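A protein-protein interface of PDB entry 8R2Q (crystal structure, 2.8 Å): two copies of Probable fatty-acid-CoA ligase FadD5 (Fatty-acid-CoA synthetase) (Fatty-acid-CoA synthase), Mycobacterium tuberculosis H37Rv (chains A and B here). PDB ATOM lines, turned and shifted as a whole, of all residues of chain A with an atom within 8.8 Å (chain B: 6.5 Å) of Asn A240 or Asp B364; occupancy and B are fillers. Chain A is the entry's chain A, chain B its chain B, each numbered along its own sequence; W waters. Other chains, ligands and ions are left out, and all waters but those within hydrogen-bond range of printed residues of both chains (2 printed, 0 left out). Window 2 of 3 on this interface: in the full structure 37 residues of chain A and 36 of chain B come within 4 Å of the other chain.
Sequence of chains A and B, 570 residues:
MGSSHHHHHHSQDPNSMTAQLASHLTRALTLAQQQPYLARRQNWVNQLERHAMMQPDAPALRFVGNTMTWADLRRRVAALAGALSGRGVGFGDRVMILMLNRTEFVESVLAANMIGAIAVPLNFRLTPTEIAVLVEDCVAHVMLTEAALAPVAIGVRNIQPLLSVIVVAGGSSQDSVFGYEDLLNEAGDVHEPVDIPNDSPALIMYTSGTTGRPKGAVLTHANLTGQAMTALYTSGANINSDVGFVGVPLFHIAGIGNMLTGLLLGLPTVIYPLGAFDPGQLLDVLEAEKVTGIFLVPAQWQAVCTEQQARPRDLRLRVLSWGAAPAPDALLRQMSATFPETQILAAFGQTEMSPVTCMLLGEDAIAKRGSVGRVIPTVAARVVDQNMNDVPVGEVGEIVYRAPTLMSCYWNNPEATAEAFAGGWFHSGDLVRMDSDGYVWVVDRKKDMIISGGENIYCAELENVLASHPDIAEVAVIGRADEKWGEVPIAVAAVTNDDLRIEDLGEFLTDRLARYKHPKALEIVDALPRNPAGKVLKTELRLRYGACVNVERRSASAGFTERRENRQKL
O of Ile A239 lies within hydrogen-bond range of NH2 of Arg B374 (3.3 Å). The guanidinium group of Arg B374 sits at hydrogen-bond distance from the side-chain amide oxygen of Asn A240. The side-chain amide nitrogen (ND2) of Asn A238 sits at hydrogen-bond distance from the side-chain carboxylate (OE2) of Glu B363, at 3.2 Å. ND2 of Asn A240 lies within hydrogen-bond range of OD2 of Asp B364 (2.7 Å).
Among the printed residues, merely in contact across the chains: Asn A240 with Leu B361, Asn A238 with Leu B361 and Asn A240 with Glu B363.
No position is printed for both chains.
Of the 14 printed residues of chain A, 3 touch a printed residue of chain B. Printed residues of chain A that touch a printed residue of chain B: Asn A238, Ile A239 and Asn A240. Among the printed residues, 7 pairs touch across the chains.
Water W1 lies within hydrogen-bond range of OD2 of Asp B364 (2.7 Å), ND2 of Asn A240 (3.4 Å), N of Leu B361 (3.4 Å) and O of Met B359 (3.4 Å). Water W2 lies within hydrogen-bond range of the side-chain amide oxygen (OD1) of Asn A240 (2.9 Å) and the guanidinium group (NE) of Arg B374 (3.3 Å).
Asn A240 touches just these residues of chain B: Leu B361, Glu B363, Asp B364 and Arg B374. Asp B364 touches just one residue of chain A: Asn A240. No residue of chain A comes within 4 Å of Gly B362. No residue of chain A comes within 4 Å of Ala B365. Printed residues of chain A within 4 Å of Glu B363: Asn A238 (3.2 Å) and Asn A240 (3.9 Å). Printed residues of chain A within 4 Å of Leu B361: Asn A238 and Asn A240. Printed residues of chain B within 4 Å of Asn A238: Leu B361 (3.7 Å) and Glu B363 (3.2 Å). Printed residues of chain B within 4 Å of Ile A239: Arg B374 (3.3 Å). Leu B360 touches none of the printed residues of chain A. The nearest residue of chain A that does not touch Asp B364 is Asn A238 (7.4 Å).
OD2 of Asp A242 is in hydrogen-bond range of N of Asn A238. The backbone NH (N) of Asn A240 lies close to the side-chain amide oxygen (OD1) of Asn A238 (3.3 Å). N of Met B359 sits at hydrogen-bond distance from O of Arg B374 (3.0 Å). The side-chain carboxylate of Asp B364 sits at hydrogen-bond distance from the side-chain hydroxyl of Tyr B439. OD1 of Asn A238 sits at hydrogen-bond distance from OG of Ser A241.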
ATOM      1  N   GLN A  55      -5.118  11.853   4.682  1.00  0.00           N
ATOM      2  CA  GLN A  55      -3.960  11.588   3.827  1.00  0.00           C
ATOM      3  C   GLN A  55      -4.105  12.394   2.544  1.00  0.00           C
ATOM      4  O   GLN A  55      -4.314  11.840   1.458  1.00  0.00           O
ATOM      5  CB  GLN A  55      -3.831  10.092   3.537  1.00  0.00           C
ATOM      6  CG  GLN A  55      -5.154   9.409   3.235  1.00  0.00           C
ATOM      7  CD  GLN A  55      -4.981   7.983   2.757  1.00  0.00           C
ATOM      8  OE1 GLN A  55      -3.871   7.450   2.739  1.00  0.00           O
ATOM      9  NE2 GLN A  55      -6.083   7.356   2.362  1.00  0.00           N
ATOM     10  N   PRO A  59      -1.668   9.014  -2.918  1.00  0.00           N
ATOM     11  CA  PRO A  59      -2.175   8.820  -4.284  1.00  0.00           C
ATOM     12  C   PRO A  59      -3.572   8.214  -4.278  1.00  0.00           C
ATOM     13  O   PRO A  59      -3.823   7.197  -3.629  1.00  0.00           O
ATOM     14  CB  PRO A  59      -1.152   7.866  -4.907  1.00  0.00           C
ATOM     15  CG  PRO A  59      -0.601   7.115  -3.752  1.00  0.00           C
ATOM     16  CD  PRO A  59      -0.567   8.087  -2.604  1.00  0.00           C
ATOM     17  N   ALA A 237      -7.362  -7.522   1.561  1.00  0.00           N
ATOM     18  CA  ALA A 237      -6.871  -6.162   1.407  1.00  0.00           C
ATOM     19  C   ALA A 237      -5.646  -5.961   2.284  1.00  0.00           C
ATOM     20  O   ALA A 237      -5.592  -6.463   3.409  1.00  0.00           O
ATOM     21  CB  ALA A 237      -7.949  -5.137   1.769  1.00  0.00           C
ATOM     22  N   ASN A 238      -4.670  -5.230   1.755  1.00  0.00           N
ATOM     23  CA  ASN A 238      -3.528  -4.740   2.520  1.00  0.00           C
ATOM     24  C   ASN A 238      -3.566  -3.221   2.438  1.00  0.00           C
ATOM     25  O   ASN A 238      -3.294  -2.646   1.378  1.00  0.00           O
ATOM     26  CB  ASN A 238      -2.214  -5.298   1.978  1.00  0.00           C
ATOM     27  CG  ASN A 238      -1.067  -5.147   2.959  1.00  0.00           C
ATOM     28  OD1 ASN A 238      -0.652  -4.032   3.286  1.00  0.00           O
ATOM     29  ND2 ASN A 238      -0.540  -6.273   3.428  1.00  0.00           N
ATOM     30  N   ILE A 239      -3.904  -2.567   3.548  1.00  0.00           N
ATOM     31  CA  ILE A 239      -4.201  -1.139   3.531  1.00  0.00           C
ATOM     32  C   ILE A 239      -2.919  -0.316   3.533  1.00  0.00           C
ATOM     33  O   ILE A 239      -2.960   0.912   3.680  1.00  0.00           O
ATOM     34  CB  ILE A 239      -5.109  -0.751   4.713  1.00  0.00           C
ATOM     35  CG1 ILE A 239      -4.435  -1.088   6.043  1.00  0.00           C
ATOM     36  CG2 ILE A 239      -6.451  -1.454   4.602  1.00  0.00           C
ATOM     37  CD1 ILE A 239      -5.318  -0.849   7.249  1.00  0.00           C
ATOM     38  N   ASN A 240      -1.776  -0.973   3.360  1.00  0.00           N
ATOM     39  CA  ASN A 240      -0.496  -0.282   3.277  1.00  0.00           C
ATOM     40  C   ASN A 240       0.144  -0.350   1.902  1.00  0.00           C
ATOM     41  O   ASN A 240       0.778   0.618   1.479  1.00  0.00           O
ATOM     42  CB  ASN A 240       0.487  -0.845   4.312  1.00  0.00           C
ATOM     43  CG  ASN A 240       0.372  -0.159   5.663  1.00  0.00           C
ATOM     44  OD1 ASN A 240      -0.231   0.910   5.784  1.00  0.00           O
ATOM     45  ND2 ASN A 240       0.965  -0.765   6.686  1.00  0.00           N
ATOM     46  N   SER A 241      -0.005  -1.466   1.184  1.00  0.00           N
ATOM     47  CA  SER A 241       0.714  -1.667  -0.067  1.00  0.00           C
ATOM     48  C   SER A 241      -0.162  -2.005  -1.267  1.00  0.00           C
ATOM     49  O   SER A 241       0.362  -2.046  -2.386  1.00  0.00           O
ATOM     50  CB  SER A 241       1.768  -2.773   0.098  1.00  0.00           C
ATOM     51  OG  SER A 241       1.168  -3.987   0.513  1.00  0.00           O
ATOM     52  N   ASP A 242      -1.459  -2.240  -1.088  1.00  0.00           N
ATOM     53  CA  ASP A 242      -2.305  -2.595  -2.220  1.00  0.00           C
ATOM     54  C   ASP A 242      -2.425  -1.435  -3.201  1.00  0.00           C
ATOM     55  O   ASP A 242      -2.522  -0.270  -2.806  1.00  0.00           O
ATOM     56  CB  ASP A 242      -3.694  -3.020  -1.745  1.00  0.00           C
ATOM     57  CG  ASP A 242      -3.751  -4.480  -1.340  1.00  0.00           C
ATOM     58  OD1 ASP A 242      -2.681  -5.122  -1.257  1.00  0.00           O
ATOM     59  OD2 ASP A 242      -4.869  -4.989  -1.112  1.00  0.00           O
ATOM     60  N   VAL A 243      -2.409  -1.766  -4.491  1.00  0.00           N
ATOM     61  CA  VAL A 243      -2.596  -0.802  -5.569  1.00  0.00           C
ATOM     62  C   VAL A 243      -3.594  -1.395  -6.552  1.00  0.00           C
ATOM     63  O   VAL A 243      -3.320  -2.431  -7.170  1.00  0.00           O
ATOM     64  CB  VAL A 243      -1.275  -0.460  -6.280  1.00  0.00           C
ATOM     65  CG1 VAL A 243      -1.535   0.467  -7.453  1.00  0.00           C
ATOM     66  CG2 VAL A 243      -0.289   0.169  -5.305  1.00  0.00           C
ATOM     67  N   LEU A 265     -11.001   2.107   1.038  1.00  0.00           N
ATOM     68  CA  LEU A 265      -9.804   1.902   1.842  1.00  0.00           C
ATOM     69  C   LEU A 265      -8.758   2.992   1.659  1.00  0.00           C
ATOM     70  O   LEU A 265      -7.718   2.944   2.322  1.00  0.00           O
ATOM     71  CB  LEU A 265      -9.181   0.544   1.515  1.00  0.00           C
ATOM     72  CG  LEU A 265     -10.121  -0.655   1.627  1.00  0.00           C
ATOM     73  CD1 LEU A 265      -9.436  -1.916   1.133  1.00  0.00           C
ATOM     74  CD2 LEU A 265     -10.598  -0.824   3.058  1.00  0.00           C
ATOM     75  N   GLY A 266      -8.997   3.962   0.783  1.00  0.00           N
ATOM     76  CA  GLY A 266      -8.019   5.012   0.569  1.00  0.00           C
ATOM     77  C   GLY A 266      -6.769   4.566  -0.154  1.00  0.00           C
ATOM     78  O   GLY A 266      -5.707   5.172   0.027  1.00  0.00           O
ATOM     79  N   LEU A 267      -6.865   3.526  -0.968  1.00  0.00           N
ATOM     80  CA  LEU A 267      -5.758   2.969  -1.722  1.00  0.00           C
ATOM     81  C   LEU A 267      -5.790   3.463  -3.163  1.00  0.00           C
ATOM     82  O   LEU A 267      -6.866   3.681  -3.730  1.00  0.00           O
ATOM     83  CB  LEU A 267      -5.815   1.439  -1.707  1.00  0.00           C
ATOM     84  CG  LEU A 267      -5.750   0.795  -0.324  1.00  0.00           C
ATOM     85  CD1 LEU A 267      -6.095  -0.680  -0.404  1.00  0.00           C
ATOM     86  CD2 LEU A 267      -4.377   0.994   0.301  1.00  0.00           C
ATOM     87  N   PRO A 268      -4.627   3.651  -3.781  1.00  0.00           N
ATOM     88  CA  PRO A 268      -4.602   4.158  -5.155  1.00  0.00           C
ATOM     89  C   PRO A 268      -5.137   3.134  -6.140  1.00  0.00           C
ATOM     90  O   PRO A 268      -5.015   1.922  -5.945  1.00  0.00           O
ATOM     91  CB  PRO A 268      -3.117   4.441  -5.400  1.00  0.00           C
ATOM     92  CG  PRO A 268      -2.409   3.508  -4.478  1.00  0.00           C
ATOM     93  CD  PRO A 268      -3.272   3.421  -3.251  1.00  0.00           C
ATOM     94  N   THR A 292      -1.151  -4.693  -7.221  1.00  0.00           N
ATOM     95  CA  THR A 292      -1.276  -5.886  -6.396  1.00  0.00           C
ATOM     96  C   THR A 292      -2.428  -6.793  -6.808  1.00  0.00           C
ATOM     97  O   THR A 292      -2.453  -7.956  -6.394  1.00  0.00           O
ATOM     98  CB  THR A 292      -1.452  -5.497  -4.923  1.00  0.00           C
ATOM     99  OG1 THR A 292      -2.630  -4.693  -4.775  1.00  0.00           O
ATOM    100  CG2 THR A 292      -0.242  -4.720  -4.433  1.00  0.00           C
ATOM    101  N   MET B 359      -4.523   0.566  13.291  1.00  0.00           N
ATOM    102  CA  MET B 359      -4.060  -0.773  12.963  1.00  0.00           C
ATOM    103  C   MET B 359      -2.572  -0.726  12.659  1.00  0.00           C
ATOM    104  O   MET B 359      -2.106   0.159  11.937  1.00  0.00           O
ATOM    105  CB  MET B 359      -4.823  -1.344  11.763  1.00  0.00           C
ATOM    106  CG  MET B 359      -4.541  -2.810  11.495  1.00  0.00           C
ATOM    107  SD  MET B 359      -5.132  -3.861  12.835  1.00  0.00           S
ATOM    108  CE  MET B 359      -6.842  -3.351  12.923  1.00  0.00           C
ATOM    109  N   LEU B 360      -1.830  -1.682  13.212  1.00  0.00           N
ATOM    110  CA  LEU B 360      -0.392  -1.794  12.994  1.00  0.00           C
ATOM    111  C   LEU B 360      -0.119  -3.126  12.308  1.00  0.00           C
ATOM    112  O   LEU B 360      -0.198  -4.184  12.942  1.00  0.00           O
ATOM    113  CB  LEU B 360       0.374  -1.683  14.312  1.00  0.00           C
ATOM    114  CG  LEU B 360       1.896  -1.802  14.229  1.00  0.00           C
ATOM    115  CD1 LEU B 360       2.471  -0.724  13.324  1.00  0.00           C
ATOM    116  CD2 LEU B 360       2.512  -1.727  15.613  1.00  0.00           C
ATOM    117  N   LEU B 361       0.190  -3.074  11.014  1.00  0.00           N
ATOM    118  CA  LEU B 361       0.526  -4.276  10.266  1.00  0.00           C
ATOM    119  C   LEU B 361       1.986  -4.648  10.502  1.00  0.00           C
ATOM    120  O   LEU B 361       2.848  -3.780  10.674  1.00  0.00           O
ATOM    121  CB  LEU B 361       0.266  -4.071   8.773  1.00  0.00           C
ATOM    122  CG  LEU B 361      -1.042  -3.372   8.384  1.00  0.00           C
ATOM    123  CD1 LEU B 361      -1.183  -3.304   6.872  1.00  0.00           C
ATOM    124  CD2 LEU B 361      -2.248  -4.060   8.998  1.00  0.00           C
ATOM    125  N   GLY B 362       2.255  -5.958  10.501  1.00  0.00           N
ATOM    126  CA  GLY B 362       3.574  -6.470  10.850  1.00  0.00           C
ATOM    127  C   GLY B 362       4.712  -5.889  10.035  1.00  0.00           C
ATOM    128  O   GLY B 362       5.867  -5.938  10.473  1.00  0.00           O
ATOM    129  N   GLU B 363       4.415  -5.336   8.857  1.00  0.00           N
ATOM    130  CA  GLU B 363       5.452  -4.696   8.060  1.00  0.00           C
ATOM    131  C   GLU B 363       6.018  -3.472   8.766  1.00  0.00           C
ATOM    132  O   GLU B 363       7.206  -3.165   8.620  1.00  0.00           O
ATOM    133  CB  GLU B 363       4.886  -4.314   6.693  1.00  0.00           C
ATOM    134  CG  GLU B 363       4.148  -5.447   6.001  1.00  0.00           C
ATOM    135  CD  GLU B 363       2.852  -4.995   5.356  1.00  0.00           C
ATOM    136  OE1 GLU B 363       2.836  -3.911   4.735  1.00  0.00           O
ATOM    137  OE2 GLU B 363       1.843  -5.723   5.481  1.00  0.00           O
ATOM    138  N   ASP B 364       5.192  -2.773   9.540  1.00  0.00           N
ATOM    139  CA  ASP B 364       5.594  -1.544  10.206  1.00  0.00           C
ATOM    140  C   ASP B 364       5.887  -1.729  11.688  1.00  0.00           C
ATOM    141  O   ASP B 364       6.314  -0.769  12.338  1.00  0.00           O
ATOM    142  CB  ASP B 364       4.505  -0.478  10.040  1.00  0.00           C
ATOM    143  CG  ASP B 364       4.062  -0.320   8.601  1.00  0.00           C
ATOM    144  OD1 ASP B 364       4.894  -0.528   7.695  1.00  0.00           O
ATOM    145  OD2 ASP B 364       2.877   0.015   8.379  1.00  0.00           O
ATOM    146  N   ALA B 365       5.679  -2.930  12.234  1.00  0.00           N
ATOM    147  CA  ALA B 365       5.902  -3.150  13.659  1.00  0.00           C
ATOM    148  C   ALA B 365       7.358  -2.953  14.059  1.00  0.00           C
ATOM    149  O   ALA B 365       7.650  -2.815  15.252  1.00  0.00           O
ATOM    150  CB  ALA B 365       5.438  -4.552  14.056  1.00  0.00           C
ATOM    151  N   ILE B 366       8.276  -2.937  13.096  1.00  0.00           N
ATOM    152  CA  ILE B 366       9.688  -2.716  13.366  1.00  0.00           C
ATOM    153  C   ILE B 366      10.123  -1.309  12.975  1.00  0.00           C
ATOM    154  O   ILE B 366      10.836  -0.646  13.731  1.00  0.00           O
ATOM    155  CB  ILE B 366      10.536  -3.783  12.643  1.00  0.00           C
ATOM    156  CG1 ILE B 366      10.158  -5.181  13.140  1.00  0.00           C
ATOM    157  CG2 ILE B 366      12.021  -3.522  12.847  1.00  0.00           C
ATOM    158  CD1 ILE B 366      10.251  -5.342  14.643  1.00  0.00           C
ATOM    159  N   ALA B 367       9.699  -0.838  11.800  1.00  0.00           N
ATOM    160  CA  ALA B 367      10.038   0.519  11.386  1.00  0.00           C
ATOM    161  C   ALA B 367       9.393   1.552  12.300  1.00  0.00           C
ATOM    162  O   ALA B 367      10.018   2.559  12.652  1.00  0.00           O
ATOM    163  CB  ALA B 367       9.615   0.746   9.935  1.00  0.00           C
ATOM    164  N   LYS B 368       8.144   1.316  12.696  1.00  0.00           N
ATOM    165  CA  LYS B 368       7.440   2.223  13.591  1.00  0.00           C
ATOM    166  C   LYS B 368       7.131   1.531  14.912  1.00  0.00           C
ATOM    167  O   LYS B 368       5.978   1.527  15.358  1.00  0.00           O
ATOM    168  CB  LYS B 368       6.147   2.720  12.939  1.00  0.00           C
ATOM    169  CG  LYS B 368       6.336   3.471  11.631  1.00  0.00           C
ATOM    170  CD  LYS B 368       6.900   4.863  11.864  1.00  0.00           C
ATOM    171  CE  LYS B 368       6.878   5.690  10.588  1.00  0.00           C
ATOM    172  NZ  LYS B 368       7.342   7.088  10.815  1.00  0.00           N
ATOM    173  N   ARG B 369       8.144   0.940  15.544  1.00  0.00           N
ATOM    174  CA  ARG B 369       7.923   0.224  16.793  1.00  0.00           C
ATOM    175  C   ARG B 369       7.467   1.184  17.886  1.00  0.00           C
ATOM    176  O   ARG B 369       7.807   2.370  17.886  1.00  0.00           O
ATOM    177  CB  ARG B 369       9.193  -0.503  17.235  1.00  0.00           C
ATOM    178  CG  ARG B 369       8.939  -1.639  18.220  1.00  0.00           C
ATOM    179  CD  ARG B 369      10.179  -1.987  19.032  1.00  0.00           C
ATOM    180  NE  ARG B 369      11.363  -2.166  18.199  1.00  0.00           N
ATOM    181  CZ  ARG B 369      12.383  -1.319  18.150  1.00  0.00           C
ATOM    182  NH1 ARG B 369      12.406  -0.221  18.887  1.00  0.00           N
ATOM    183  NH2 ARG B 369      13.407  -1.584  17.343  1.00  0.00           N
ATOM    184  N   SER B 371       4.542   2.264  18.147  1.00  0.00           N
ATOM    185  CA  SER B 371       3.343   2.919  17.660  1.00  0.00           C
ATOM    186  C   SER B 371       2.154   1.961  17.704  1.00  0.00           C
ATOM    187  O   SER B 371       2.305   0.743  17.831  1.00  0.00           O
ATOM    188  CB  SER B 371       3.554   3.426  16.233  1.00  0.00           C
ATOM    189  OG  SER B 371       2.318   3.673  15.588  1.00  0.00           O
ATOM    190  N   ARG B 374      -1.542   3.264  12.020  1.00  0.00           N
ATOM    191  CA  ARG B 374      -2.198   4.393  11.381  1.00  0.00           C
ATOM    192  C   ARG B 374      -3.707   4.268  11.547  1.00  0.00           C
ATOM    193  O   ARG B 374      -4.243   3.175  11.748  1.00  0.00           O
ATOM    194  CB  ARG B 374      -1.834   4.482   9.892  1.00  0.00           C
ATOM    195  CG  ARG B 374      -0.340   4.611   9.639  1.00  0.00           C
ATOM    196  CD  ARG B 374      -0.013   5.052   8.215  1.00  0.00           C
ATOM    197  NE  ARG B 374      -0.388   4.065   7.210  1.00  0.00           N
ATOM    198  CZ  ARG B 374      -1.079   4.341   6.114  1.00  0.00           C
ATOM    199  NH1 ARG B 374      -1.473   5.573   5.837  1.00  0.00           N
ATOM    200  NH2 ARG B 374      -1.375   3.357   5.268  1.00  0.00           N
ATOM    201  N   TYR B 439       1.407   7.963  11.449  1.00  0.00           N
ATOM    202  CA  TYR B 439       1.432   6.967  12.508  1.00  0.00           C
ATOM    203  C   TYR B 439       1.141   7.607  13.860  1.00  0.00           C
ATOM    204  O   TYR B 439       1.503   8.758  14.123  1.00  0.00           O
ATOM    205  CB  TYR B 439       2.778   6.246  12.536  1.00  0.00           C
ATOM    206  CG  TYR B 439       2.923   5.253  11.410  1.00  0.00           C
ATOM    207  CD1 TYR B 439       3.310   5.664  10.143  1.00  0.00           C
ATOM    208  CD2 TYR B 439       2.649   3.906  11.607  1.00  0.00           C
ATOM    209  CE1 TYR B 439       3.432   4.762   9.107  1.00  0.00           C
ATOM    210  CE2 TYR B 439       2.769   2.994  10.577  1.00  0.00           C
ATOM    211  CZ  TYR B 439       3.160   3.429   9.329  1.00  0.00           C
ATOM    212  OH  TYR B 439       3.281   2.529   8.297  1.00  0.00           O
HETATM  213  O   HOH W   1       0.692   0.111   9.952  1.00  0.00           O
HETATM  214  O   HOH W   2      -1.159   1.091   8.493  1.00  0.00           O
